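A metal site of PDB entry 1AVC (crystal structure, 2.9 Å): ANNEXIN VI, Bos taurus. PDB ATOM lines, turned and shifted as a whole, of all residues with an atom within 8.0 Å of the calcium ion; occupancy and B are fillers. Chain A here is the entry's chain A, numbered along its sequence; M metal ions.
The calcium ion is bound by the backbone carbonyl oxygen (O) of Gly 380 (2.5 Å), the side-chain carboxylate (OE1) of Glu 420 (2.5 Å), the backbone carbonyl oxygen (O) of Leu 379 (2.5 Å), the backbone carbonyl oxygen (O) of Gly 378 (2.7 Å) and the side-chain carboxylate (OE2) of Glu 420 (2.9 Å).
The calcium ion has five donor atoms within binding distance.
Slightly farther from the calcium ion lies O of Met 376 (3.0 Å).
Merely in contact with the calcium ion: Thr 381 (3.6 Å).
The nearest printed residue that does not touch the calcium ion is Lys 377 (4.2 Å).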
ATOM      1  N   ARG A 373      -3.272  -5.006  -5.670  1.00  0.00           N
ATOM      2  CA  ARG A 373      -3.019  -5.828  -4.490  1.00  0.00           C
ATOM      3  C   ARG A 373      -3.313  -7.298  -4.784  1.00  0.00           C
ATOM      4  O   ARG A 373      -2.568  -8.189  -4.359  1.00  0.00           O
ATOM      5  CB  ARG A 373      -3.899  -5.356  -3.327  1.00  0.00           C
ATOM      6  CG  ARG A 373      -3.977  -6.329  -2.167  1.00  0.00           C
ATOM      7  CD  ARG A 373      -2.979  -5.964  -1.072  1.00  0.00           C
ATOM      8  NE  ARG A 373      -2.933  -6.971  -0.022  1.00  0.00           N
ATOM      9  CZ  ARG A 373      -1.890  -7.169   0.779  1.00  0.00           C
ATOM     10  NH1 ARG A 373      -0.791  -6.426   0.636  1.00  0.00           N
ATOM     11  NH2 ARG A 373      -1.930  -8.107   1.717  1.00  0.00           N
ATOM     12  N   LYS A 374      -4.388  -7.545  -5.530  1.00  0.00           N
ATOM     13  CA  LYS A 374      -4.784  -8.891  -5.889  1.00  0.00           C
ATOM     14  C   LYS A 374      -3.766  -9.558  -6.814  1.00  0.00           C
ATOM     15  O   LYS A 374      -3.422 -10.729  -6.634  1.00  0.00           O
ATOM     16  CB  LYS A 374      -6.153  -8.870  -6.577  1.00  0.00           C
ATOM     17  CG  LYS A 374      -6.626 -10.217  -7.118  1.00  0.00           C
ATOM     18  CD  LYS A 374      -6.179 -10.429  -8.567  1.00  0.00           C
ATOM     19  CE  LYS A 374      -6.757  -9.372  -9.496  1.00  0.00           C
ATOM     20  NZ  LYS A 374      -6.218  -9.500 -10.871  1.00  0.00           N
ATOM     21  N   ALA A 375      -3.284  -8.809  -7.802  1.00  0.00           N
ATOM     22  CA  ALA A 375      -2.327  -9.323  -8.772  1.00  0.00           C
ATOM     23  C   ALA A 375      -0.915  -9.502  -8.217  1.00  0.00           C
ATOM     24  O   ALA A 375      -0.001  -9.871  -8.956  1.00  0.00           O
ATOM     25  CB  ALA A 375      -2.287  -8.408  -9.987  1.00  0.00           C
ATOM     26  N   MET A 376      -0.728  -9.256  -6.925  1.00  0.00           N
ATOM     27  CA  MET A 376       0.580  -9.397  -6.313  1.00  0.00           C
ATOM     28  C   MET A 376       0.591 -10.468  -5.225  1.00  0.00           C
ATOM     29  O   MET A 376       1.650 -10.931  -4.802  1.00  0.00           O
ATOM     30  CB  MET A 376       1.037  -8.060  -5.725  1.00  0.00           C
ATOM     31  CG  MET A 376       1.387  -7.013  -6.768  1.00  0.00           C
ATOM     32  SD  MET A 376       2.175  -5.561  -6.056  1.00  0.00           S
ATOM     33  CE  MET A 376       0.794  -4.443  -5.929  1.00  0.00           C
ATOM     34  N   LYS A 377      -0.602 -10.860  -4.776  1.00  0.00           N
ATOM     35  CA  LYS A 377      -0.730 -11.871  -3.734  1.00  0.00           C
ATOM     36  C   LYS A 377      -0.398 -13.251  -4.284  1.00  0.00           C
ATOM     37  O   LYS A 377      -0.622 -13.532  -5.469  1.00  0.00           O
ATOM     38  CB  LYS A 377      -2.146 -11.866  -3.169  1.00  0.00           C
ATOM     39  CG  LYS A 377      -2.258 -11.267  -1.779  1.00  0.00           C
ATOM     40  CD  LYS A 377      -3.236 -10.093  -1.757  1.00  0.00           C
ATOM     41  CE  LYS A 377      -4.241 -10.236  -0.622  1.00  0.00           C
ATOM     42  NZ  LYS A 377      -5.619  -9.848  -1.050  1.00  0.00           N
ATOM     43  N   GLY A 378       0.128 -14.124  -3.425  1.00  0.00           N
ATOM     44  CA  GLY A 378       0.487 -15.469  -3.838  1.00  0.00           C
ATOM     45  C   GLY A 378       1.973 -15.552  -4.110  1.00  0.00           C
ATOM     46  O   GLY A 378       2.716 -14.623  -3.809  1.00  0.00           O
ATOM     47  N   LEU A 379       2.425 -16.672  -4.683  1.00  0.00           N
ATOM     48  CA  LEU A 379       3.842 -16.819  -4.997  1.00  0.00           C
ATOM     49  C   LEU A 379       4.161 -16.002  -6.243  1.00  0.00           C
ATOM     50  O   LEU A 379       4.997 -15.093  -6.195  1.00  0.00           O
ATOM     51  CB  LEU A 379       4.193 -18.294  -5.246  1.00  0.00           C
ATOM     52  CG  LEU A 379       5.701 -18.588  -5.278  1.00  0.00           C
ATOM     53  CD1 LEU A 379       6.314 -18.246  -3.930  1.00  0.00           C
ATOM     54  CD2 LEU A 379       5.942 -20.042  -5.625  1.00  0.00           C
ATOM     55  N   GLY A 380       3.495 -16.339  -7.339  1.00  0.00           N
ATOM     56  CA  GLY A 380       3.694 -15.632  -8.589  1.00  0.00           C
ATOM     57  C   GLY A 380       3.019 -14.278  -8.568  1.00  0.00           C
ATOM     58  O   GLY A 380       2.156 -14.014  -7.727  1.00  0.00           O
ATOM     59  N   THR A 381       3.394 -13.413  -9.500  1.00  0.00           N
ATOM     60  CA  THR A 381       2.821 -12.076  -9.578  1.00  0.00           C
ATOM     61  C   THR A 381       2.118 -11.838 -10.908  1.00  0.00           C
ATOM     62  O   THR A 381       2.742 -11.898 -11.965  1.00  0.00           O
ATOM     63  CB  THR A 381       3.922 -11.007  -9.392  1.00  0.00           C
ATOM     64  OG1 THR A 381       3.643  -9.877 -10.228  1.00  0.00           O
ATOM     65  CG2 THR A 381       5.277 -11.584  -9.758  1.00  0.00           C
ATOM     66  N   ASP A 382       0.820 -11.569 -10.858  1.00  0.00           N
ATOM     67  CA  ASP A 382       0.038 -11.316 -12.068  1.00  0.00           C
ATOM     68  C   ASP A 382       0.510  -9.983 -12.654  1.00  0.00           C
ATOM     69  O   ASP A 382       0.037  -8.920 -12.276  1.00  0.00           O
ATOM     70  CB  ASP A 382      -1.444 -11.231 -11.726  1.00  0.00           C
ATOM     71  CG  ASP A 382      -2.311 -10.880 -12.927  1.00  0.00           C
ATOM     72  OD1 ASP A 382      -1.757 -10.723 -14.037  1.00  0.00           O
ATOM     73  OD2 ASP A 382      -3.540 -10.755 -12.751  1.00  0.00           O
ATOM     74  N   SER A 419       9.351  -5.292  -5.014  1.00  0.00           N
ATOM     75  CA  SER A 419       9.606  -6.665  -4.577  1.00  0.00           C
ATOM     76  C   SER A 419       8.950  -7.740  -5.442  1.00  0.00           C
ATOM     77  O   SER A 419       9.546  -8.794  -5.677  1.00  0.00           O
ATOM     78  CB  SER A 419       9.162  -6.835  -3.127  1.00  0.00           C
ATOM     79  OG  SER A 419       8.427  -8.026  -2.944  1.00  0.00           O
ATOM     80  N   GLU A 420       7.733  -7.487  -5.911  1.00  0.00           N
ATOM     81  CA  GLU A 420       7.023  -8.464  -6.722  1.00  0.00           C
ATOM     82  C   GLU A 420       7.417  -8.434  -8.202  1.00  0.00           C
ATOM     83  O   GLU A 420       7.161  -9.388  -8.940  1.00  0.00           O
ATOM     84  CB  GLU A 420       5.525  -8.269  -6.561  1.00  0.00           C
ATOM     85  CG  GLU A 420       4.998  -8.887  -5.295  1.00  0.00           C
ATOM     86  CD  GLU A 420       4.745 -10.363  -5.481  1.00  0.00           C
ATOM     87  OE1 GLU A 420       4.046 -10.705  -6.448  1.00  0.00           O
ATOM     88  OE2 GLU A 420       5.246 -11.169  -4.680  1.00  0.00           O
ATOM     89  N   LEU A 421       8.039  -7.338  -8.631  1.00  0.00           N
ATOM     90  CA  LEU A 421       8.470  -7.214 -10.028  1.00  0.00           C
ATOM     91  C   LEU A 421       9.990  -7.290 -10.128  1.00  0.00           C
ATOM     92  O   LEU A 421      10.701  -7.068  -9.142  1.00  0.00           O
ATOM     93  CB  LEU A 421       7.989  -5.884 -10.608  1.00  0.00           C
ATOM     94  CG  LEU A 421       6.483  -5.736 -10.891  1.00  0.00           C
ATOM     95  CD1 LEU A 421       6.243  -4.477 -11.714  1.00  0.00           C
ATOM     96  CD2 LEU A 421       5.974  -6.962 -11.640  1.00  0.00           C
HETATM   97 CA    CA M   1       3.511 -13.072  -5.916  1.00  0.00          CA
